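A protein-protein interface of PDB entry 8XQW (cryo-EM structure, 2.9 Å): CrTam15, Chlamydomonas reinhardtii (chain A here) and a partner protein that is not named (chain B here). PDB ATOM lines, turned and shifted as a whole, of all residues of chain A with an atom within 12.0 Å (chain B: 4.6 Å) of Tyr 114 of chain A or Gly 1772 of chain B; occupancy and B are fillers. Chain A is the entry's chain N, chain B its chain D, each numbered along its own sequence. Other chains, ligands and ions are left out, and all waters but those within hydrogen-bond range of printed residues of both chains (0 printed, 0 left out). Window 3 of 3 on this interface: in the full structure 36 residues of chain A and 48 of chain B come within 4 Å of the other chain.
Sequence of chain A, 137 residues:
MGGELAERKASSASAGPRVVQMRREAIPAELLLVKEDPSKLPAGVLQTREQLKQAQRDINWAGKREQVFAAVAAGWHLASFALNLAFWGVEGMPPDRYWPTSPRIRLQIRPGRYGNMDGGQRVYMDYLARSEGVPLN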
ATOM      1  N   ILE A 109      17.571   5.708 -26.613  1.00  0.00           N
ATOM      2  CA  ILE A 109      16.955   4.411 -26.866  1.00  0.00           C
ATOM      3  C   ILE A 109      17.078   3.561 -25.611  1.00  0.00           C
ATOM      4  O   ILE A 109      18.166   3.454 -25.033  1.00  0.00           O
ATOM      5  CB  ILE A 109      17.608   3.713 -28.067  1.00  0.00           C
ATOM      6  CG1 ILE A 109      17.090   4.311 -29.369  1.00  0.00           C
ATOM      7  CG2 ILE A 109      17.344   2.238 -28.024  1.00  0.00           C
ATOM      8  CD1 ILE A 109      17.564   3.586 -30.590  1.00  0.00           C
ATOM      9  N   ARG A 110      15.968   2.957 -25.193  1.00  0.00           N
ATOM     10  CA  ARG A 110      15.959   2.098 -24.018  1.00  0.00           C
ATOM     11  C   ARG A 110      14.773   1.151 -24.116  1.00  0.00           C
ATOM     12  O   ARG A 110      13.811   1.450 -24.831  1.00  0.00           O
ATOM     13  CB  ARG A 110      15.883   2.928 -22.732  1.00  0.00           C
ATOM     14  CG  ARG A 110      14.773   3.948 -22.707  1.00  0.00           C
ATOM     15  CD  ARG A 110      14.796   4.738 -21.406  1.00  0.00           C
ATOM     16  NE  ARG A 110      14.450   3.919 -20.246  1.00  0.00           N
ATOM     17  CZ  ARG A 110      15.331   3.317 -19.452  1.00  0.00           C
ATOM     18  NH1 ARG A 110      16.631   3.432 -19.682  1.00  0.00           N
ATOM     19  NH2 ARG A 110      14.912   2.597 -18.423  1.00  0.00           N
ATOM     20  N   PRO A 111      14.809   0.011 -23.425  1.00  0.00           N
ATOM     21  CA  PRO A 111      13.735  -0.975 -23.572  1.00  0.00           C
ATOM     22  C   PRO A 111      12.442  -0.521 -22.910  1.00  0.00           C
ATOM     23  O   PRO A 111      12.386   0.487 -22.204  1.00  0.00           O
ATOM     24  CB  PRO A 111      14.299  -2.222 -22.881  1.00  0.00           C
ATOM     25  CG  PRO A 111      15.761  -1.963 -22.728  1.00  0.00           C
ATOM     26  CD  PRO A 111      15.886  -0.496 -22.563  1.00  0.00           C
ATOM     27  N   GLY A 112      11.385  -1.293 -23.155  1.00  0.00           N
ATOM     28  CA  GLY A 112      10.077  -1.002 -22.602  1.00  0.00           C
ATOM     29  C   GLY A 112       9.604  -2.038 -21.605  1.00  0.00           C
ATOM     30  O   GLY A 112      10.363  -2.445 -20.721  1.00  0.00           O
ATOM     31  N   ARG A 113       8.351  -2.478 -21.732  1.00  0.00           N
ATOM     32  CA  ARG A 113       7.806  -3.494 -20.844  1.00  0.00           C
ATOM     33  C   ARG A 113       7.627  -4.850 -21.504  1.00  0.00           C
ATOM     34  O   ARG A 113       7.749  -5.869 -20.818  1.00  0.00           O
ATOM     35  CB  ARG A 113       6.451  -3.052 -20.277  1.00  0.00           C
ATOM     36  CG  ARG A 113       6.504  -1.769 -19.479  1.00  0.00           C
ATOM     37  CD  ARG A 113       5.268  -1.607 -18.614  1.00  0.00           C
ATOM     38  NE  ARG A 113       4.056  -2.075 -19.281  1.00  0.00           N
ATOM     39  CZ  ARG A 113       2.822  -1.756 -18.903  1.00  0.00           C
ATOM     40  NH1 ARG A 113       2.626  -0.955 -17.864  1.00  0.00           N
ATOM     41  NH2 ARG A 113       1.780  -2.233 -19.568  1.00  0.00           N
ATOM     42  N   TYR A 114       7.345  -4.891 -22.795  1.00  0.00           N
ATOM     43  CA  TYR A 114       7.152  -6.145 -23.503  1.00  0.00           C
ATOM     44  C   TYR A 114       8.433  -6.540 -24.225  1.00  0.00           C
ATOM     45  O   TYR A 114       9.401  -5.782 -24.285  1.00  0.00           O
ATOM     46  CB  TYR A 114       5.994  -6.038 -24.495  1.00  0.00           C
ATOM     47  CG  TYR A 114       4.732  -5.463 -23.894  1.00  0.00           C
ATOM     48  CD1 TYR A 114       4.558  -4.096 -23.777  1.00  0.00           C
ATOM     49  CD2 TYR A 114       3.714  -6.290 -23.448  1.00  0.00           C
ATOM     50  CE1 TYR A 114       3.411  -3.568 -23.233  1.00  0.00           C
ATOM     51  CE2 TYR A 114       2.561  -5.769 -22.905  1.00  0.00           C
ATOM     52  CZ  TYR A 114       2.417  -4.406 -22.799  1.00  0.00           C
ATOM     53  OH  TYR A 114       1.275  -3.871 -22.256  1.00  0.00           O
ATOM     54  N   GLY A 115       8.430  -7.753 -24.765  1.00  0.00           N
ATOM     55  CA  GLY A 115       9.594  -8.262 -25.452  1.00  0.00           C
ATOM     56  C   GLY A 115      10.770  -8.585 -24.564  1.00  0.00           C
ATOM     57  O   GLY A 115      11.851  -8.884 -25.081  1.00  0.00           O
ATOM     58  N   ASN A 116      10.598  -8.542 -23.250  1.00  0.00           N
ATOM     59  CA  ASN A 116      11.674  -8.795 -22.300  1.00  0.00           C
ATOM     60  C   ASN A 116      11.396 -10.122 -21.602  1.00  0.00           C
ATOM     61  O   ASN A 116      10.582 -10.197 -20.682  1.00  0.00           O
ATOM     62  CB  ASN A 116      11.789  -7.658 -21.302  1.00  0.00           C
ATOM     63  CG  ASN A 116      13.213  -7.409 -20.874  1.00  0.00           C
ATOM     64  OD1 ASN A 116      13.992  -8.346 -20.707  1.00  0.00           O
ATOM     65  ND2 ASN A 116      13.567  -6.143 -20.703  1.00  0.00           N
ATOM     66  N   MET A 117      12.071 -11.175 -22.053  1.00  0.00           N
ATOM     67  CA  MET A 117      11.968 -12.480 -21.423  1.00  0.00           C
ATOM     68  C   MET A 117      13.098 -12.658 -20.419  1.00  0.00           C
ATOM     69  O   MET A 117      14.179 -12.085 -20.575  1.00  0.00           O
ATOM     70  CB  MET A 117      12.021 -13.596 -22.467  1.00  0.00           C
ATOM     71  CG  MET A 117      11.082 -13.406 -23.640  1.00  0.00           C
ATOM     72  SD  MET A 117       9.350 -13.441 -23.163  1.00  0.00           S
ATOM     73  CE  MET A 117       8.589 -12.754 -24.628  1.00  0.00           C
ATOM     74  N   ASP A 118      12.840 -13.451 -19.382  1.00  0.00           N
ATOM     75  CA  ASP A 118      13.884 -13.734 -18.404  1.00  0.00           C
ATOM     76  C   ASP A 118      14.898 -14.738 -18.926  1.00  0.00           C
ATOM     77  O   ASP A 118      15.935 -14.945 -18.287  1.00  0.00           O
ATOM     78  CB  ASP A 118      13.268 -14.248 -17.104  1.00  0.00           C
ATOM     79  CG  ASP A 118      13.949 -13.683 -15.877  1.00  0.00           C
ATOM     80  OD1 ASP A 118      15.196 -13.608 -15.867  1.00  0.00           O
ATOM     81  OD2 ASP A 118      13.235 -13.309 -14.923  1.00  0.00           O
ATOM     82  N   GLY A 119      14.623 -15.372 -20.060  1.00  0.00           N
ATOM     83  CA  GLY A 119      15.566 -16.302 -20.638  1.00  0.00           C
ATOM     84  C   GLY A 119      16.435 -15.663 -21.696  1.00  0.00           C
ATOM     85  O   GLY A 119      17.214 -16.345 -22.366  1.00  0.00           O
ATOM     86  N   GLY A 120      16.313 -14.344 -21.852  1.00  0.00           N
ATOM     87  CA  GLY A 120      17.070 -13.656 -22.880  1.00  0.00           C
ATOM     88  C   GLY A 120      18.495 -13.343 -22.487  1.00  0.00           C
ATOM     89  O   GLY A 120      19.402 -13.440 -23.320  1.00  0.00           O
ATOM     90  N   LEU B1765       5.828  -6.555 -31.674  1.00  0.00           N
ATOM     91  CA  LEU B1765       5.892  -5.768 -30.451  1.00  0.00           C
ATOM     92  C   LEU B1765       4.826  -4.684 -30.430  1.00  0.00           C
ATOM     93  O   LEU B1765       4.265  -4.382 -29.373  1.00  0.00           O
ATOM     94  CB  LEU B1765       7.276  -5.151 -30.299  1.00  0.00           C
ATOM     95  CG  LEU B1765       8.316  -5.931 -29.504  1.00  0.00           C
ATOM     96  CD1 LEU B1765       7.885  -6.030 -28.069  1.00  0.00           C
ATOM     97  CD2 LEU B1765       8.536  -7.310 -30.089  1.00  0.00           C
ATOM     98  N   ARG B1768       1.648  -6.359 -29.536  1.00  0.00           N
ATOM     99  CA  ARG B1768       1.682  -6.691 -28.117  1.00  0.00           C
ATOM    100  C   ARG B1768       1.392  -5.467 -27.263  1.00  0.00           C
ATOM    101  O   ARG B1768       0.660  -5.557 -26.275  1.00  0.00           O
ATOM    102  CB  ARG B1768       3.035  -7.282 -27.736  1.00  0.00           C
ATOM    103  CG  ARG B1768       3.199  -8.732 -28.097  1.00  0.00           C
ATOM    104  CD  ARG B1768       4.365  -9.325 -27.350  1.00  0.00           C
ATOM    105  NE  ARG B1768       5.175 -10.177 -28.208  1.00  0.00           N
ATOM    106  CZ  ARG B1768       6.388 -10.611 -27.890  1.00  0.00           C
ATOM    107  NH1 ARG B1768       6.931 -10.270 -26.733  1.00  0.00           N
ATOM    108  NH2 ARG B1768       7.057 -11.384 -28.731  1.00  0.00           N
ATOM    109  N   GLN B1769       1.952  -4.316 -27.630  1.00  0.00           N
ATOM    110  CA  GLN B1769       1.664  -3.096 -26.886  1.00  0.00           C
ATOM    111  C   GLN B1769       0.181  -2.761 -26.936  1.00  0.00           C
ATOM    112  O   GLN B1769      -0.430  -2.471 -25.902  1.00  0.00           O
ATOM    113  CB  GLN B1769       2.489  -1.933 -27.434  1.00  0.00           C
ATOM    114  CG  GLN B1769       3.894  -1.842 -26.865  1.00  0.00           C
ATOM    115  CD  GLN B1769       4.802  -0.945 -27.687  1.00  0.00           C
ATOM    116  OE1 GLN B1769       4.369   0.071 -28.231  1.00  0.00           O
ATOM    117  NE2 GLN B1769       6.071  -1.324 -27.787  1.00  0.00           N
ATOM    118  N   GLU B1770      -0.417  -2.795 -28.126  1.00  0.00           N
ATOM    119  CA  GLU B1770      -1.834  -2.457 -28.242  1.00  0.00           C
ATOM    120  C   GLU B1770      -2.701  -3.399 -27.412  1.00  0.00           C
ATOM    121  O   GLU B1770      -3.597  -2.959 -26.679  1.00  0.00           O
ATOM    122  CB  GLU B1770      -2.261  -2.483 -29.707  1.00  0.00           C
ATOM    123  CG  GLU B1770      -2.443  -1.114 -30.352  1.00  0.00           C
ATOM    124  CD  GLU B1770      -1.148  -0.331 -30.524  1.00  0.00           C
ATOM    125  OE1 GLU B1770      -0.071  -0.833 -30.151  1.00  0.00           O
ATOM    126  OE2 GLU B1770      -1.211   0.803 -31.042  1.00  0.00           O
ATOM    127  N   LYS B1771      -2.438  -4.704 -27.508  1.00  0.00           N
ATOM    128  CA  LYS B1771      -3.224  -5.675 -26.755  1.00  0.00           C
ATOM    129  C   LYS B1771      -3.017  -5.517 -25.255  1.00  0.00           C
ATOM    130  O   LYS B1771      -3.961  -5.665 -24.472  1.00  0.00           O
ATOM    131  CB  LYS B1771      -2.862  -7.090 -27.195  1.00  0.00           C
ATOM    132  CG  LYS B1771      -3.332  -7.450 -28.589  1.00  0.00           C
ATOM    133  CD  LYS B1771      -2.446  -8.519 -29.203  1.00  0.00           C
ATOM    134  CE  LYS B1771      -3.195  -9.305 -30.250  1.00  0.00           C
ATOM    135  NZ  LYS B1771      -4.058  -8.424 -31.075  1.00  0.00           N
ATOM    136  N   GLY B1772      -1.789  -5.209 -24.836  1.00  0.00           N
ATOM    137  CA  GLY B1772      -1.530  -4.990 -23.425  1.00  0.00           C
ATOM    138  C   GLY B1772      -2.253  -3.778 -22.876  1.00  0.00           C
ATOM    139  O   GLY B1772      -2.771  -3.813 -21.762  1.00  0.00           O
ATOM    140  N   THR B1773      -2.305  -2.690 -23.647  1.00  0.00           N
ATOM    141  CA  THR B1773      -3.080  -1.536 -23.195  1.00  0.00           C
ATOM    142  C   THR B1773      -4.569  -1.845 -23.161  1.00  0.00           C
ATOM    143  O   THR B1773      -5.291  -1.357 -22.286  1.00  0.00           O
ATOM    144  CB  THR B1773      -2.820  -0.311 -24.071  1.00  0.00           C
ATOM    145  OG1 THR B1773      -3.539  -0.435 -25.307  1.00  0.00           O
ATOM    146  CG2 THR B1773      -1.339  -0.118 -24.312  1.00  0.00           C
ATOM    147  N   LEU B1774      -5.054  -2.650 -24.105  1.00  0.00           N
ATOM    148  CA  LEU B1774      -6.475  -2.982 -24.076  1.00  0.00           C
ATOM    149  C   LEU B1774      -6.813  -3.857 -22.877  1.00  0.00           C
ATOM    150  O   LEU B1774      -7.888  -3.723 -22.283  1.00  0.00           O
ATOM    151  CB  LEU B1774      -6.888  -3.673 -25.369  1.00  0.00           C
ATOM    152  CG  LEU B1774      -8.370  -4.033 -25.394  1.00  0.00           C
ATOM    153  CD1 LEU B1774      -9.070  -3.362 -26.566  1.00  0.00           C
ATOM    154  CD2 LEU B1774      -8.544  -5.538 -25.431  1.00  0.00           C
ATOM    155  N   PHE B1775      -5.904  -4.752 -22.498  1.00  0.00           N
ATOM    156  CA  PHE B1775      -6.208  -5.686 -21.423  1.00  0.00           C
ATOM    157  C   PHE B1775      -5.881  -5.126 -20.045  1.00  0.00           C
ATOM    158  O   PHE B1775      -6.443  -5.593 -19.050  1.00  0.00           O
ATOM    159  CB  PHE B1775      -5.452  -6.994 -21.632  1.00  0.00           C
ATOM    160  CG  PHE B1775      -6.222  -8.013 -22.404  1.00  0.00           C
ATOM    161  CD1 PHE B1775      -7.595  -8.116 -22.258  1.00  0.00           C
ATOM    162  CD2 PHE B1775      -5.576  -8.870 -23.271  1.00  0.00           C
ATOM    163  CE1 PHE B1775      -8.305  -9.051 -22.965  1.00  0.00           C
ATOM    164  CE2 PHE B1775      -6.280  -9.807 -23.980  1.00  0.00           C
ATOM    165  CZ  PHE B1775      -7.647  -9.899 -23.827  1.00  0.00           C
ATOM    166  N   TRP B1776      -4.983  -4.147 -19.953  1.00  0.00           N
ATOM    167  CA  TRP B1776      -4.464  -3.703 -18.663  1.00  0.00           C
ATOM    168  C   TRP B1776      -4.715  -2.224 -18.393  1.00  0.00           C
ATOM    169  O   TRP B1776      -4.761  -1.805 -17.233  1.00  0.00           O
ATOM    170  CB  TRP B1776      -2.967  -4.022 -18.579  1.00  0.00           C
ATOM    171  CG  TRP B1776      -2.688  -5.263 -17.800  1.00  0.00           C
ATOM    172  CD1 TRP B1776      -3.057  -5.516 -16.516  1.00  0.00           C
ATOM    173  CD2 TRP B1776      -2.032  -6.445 -18.267  1.00  0.00           C
ATOM    174  NE1 TRP B1776      -2.646  -6.766 -16.139  1.00  0.00           N
ATOM    175  CE2 TRP B1776      -2.018  -7.361 -17.198  1.00  0.00           C
ATOM    176  CE3 TRP B1776      -1.447  -6.814 -19.480  1.00  0.00           C
ATOM    177  CZ2 TRP B1776      -1.443  -8.625 -17.305  1.00  0.00           C
ATOM    178  CZ3 TRP B1776      -0.875  -8.068 -19.584  1.00  0.00           C
ATOM    179  CH2 TRP B1776      -0.879  -8.958 -18.503  1.00  0.00           C
ATOM    180  N   ASP B1777      -4.854  -1.412 -19.436  1.00  0.00           N
ATOM    181  CA  ASP B1777      -5.083   0.004 -19.188  1.00  0.00           C
ATOM    182  C   ASP B1777      -6.552   0.331 -18.967  1.00  0.00           C
ATOM    183  O   ASP B1777      -6.857   1.398 -18.428  1.00  0.00           O
ATOM    184  CB  ASP B1777      -4.515   0.845 -20.332  1.00  0.00           C
ATOM    185  CG  ASP B1777      -2.993   0.932 -20.290  1.00  0.00           C
ATOM    186  OD1 ASP B1777      -2.409   0.588 -19.240  1.00  0.00           O
ATOM    187  OD2 ASP B1777      -2.385   1.352 -21.299  1.00  0.00           O
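NH2 of Arg 113 of chain A is in hydrogen-bond range of OH of Tyr 114 of chain A (3.2 Å).
Leu 1765 of chain B touches Tyr 114 of chain A. Tyr 114 of chain A touches Arg 1768 of chain B. CD1 of Tyr 114 of chain A touches CG of Gln 1769 of chain B, 3.9 Å away. Tyr 114 of chain A touches Gly 1772 of chain B (OH to CA, 3.2 Å). N of Gly 115 of chain A touches CD1 of Leu 1765 of chain B, at 3.8 Å. Gly 115 of chain A touches Arg 1768 of chain B (N to NH1, 3.5 Å). Met 117 of chain A touches Arg 1768 of chain B.
Hydrophobic or aromatic side chains of chain A that line the printed part of chain B: Tyr 114 and Met 117. Printed residues of chain B that touch a printed residue of chain A: Leu 1765, Arg 1768, Gln 1769 and Gly 1772. Among the printed residues, no Asp or Glu carboxylate lies within 4 Å of a Lys or Arg side-chain nitrogen of the other chain.
Of the printed residues of chain B, Tyr 114 of chain A touches Leu 1765, Arg 1768, Gln 1769 and Gly 1772. Printed residues of chain A within 4 Å of Gly 1772 of chain B: Tyr 114 (3.2 Å). Leu 1765 of chain B touches two residues of chain A. Gln 1769 of chain B touches one residue of chain A. No residue of chain A comes within 4 Å of Lys 1771 of chain B. No residue of chain A comes within 4 Å of Leu 1774 of chain B. No residue of chain A comes within 4 Å of Phe 1775 of chain B. Of the printed residues of chain B, Met 117 of chain A touches Arg 1768 (3.7 Å). Printed residues of chain B within 4 Å of Gly 115 of chain A: Leu 1765 and Arg 1768. The nearest printed residue of chain B that does not touch Gly 115 of chain A is Gln 1769 of chain B (7.5 Å).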
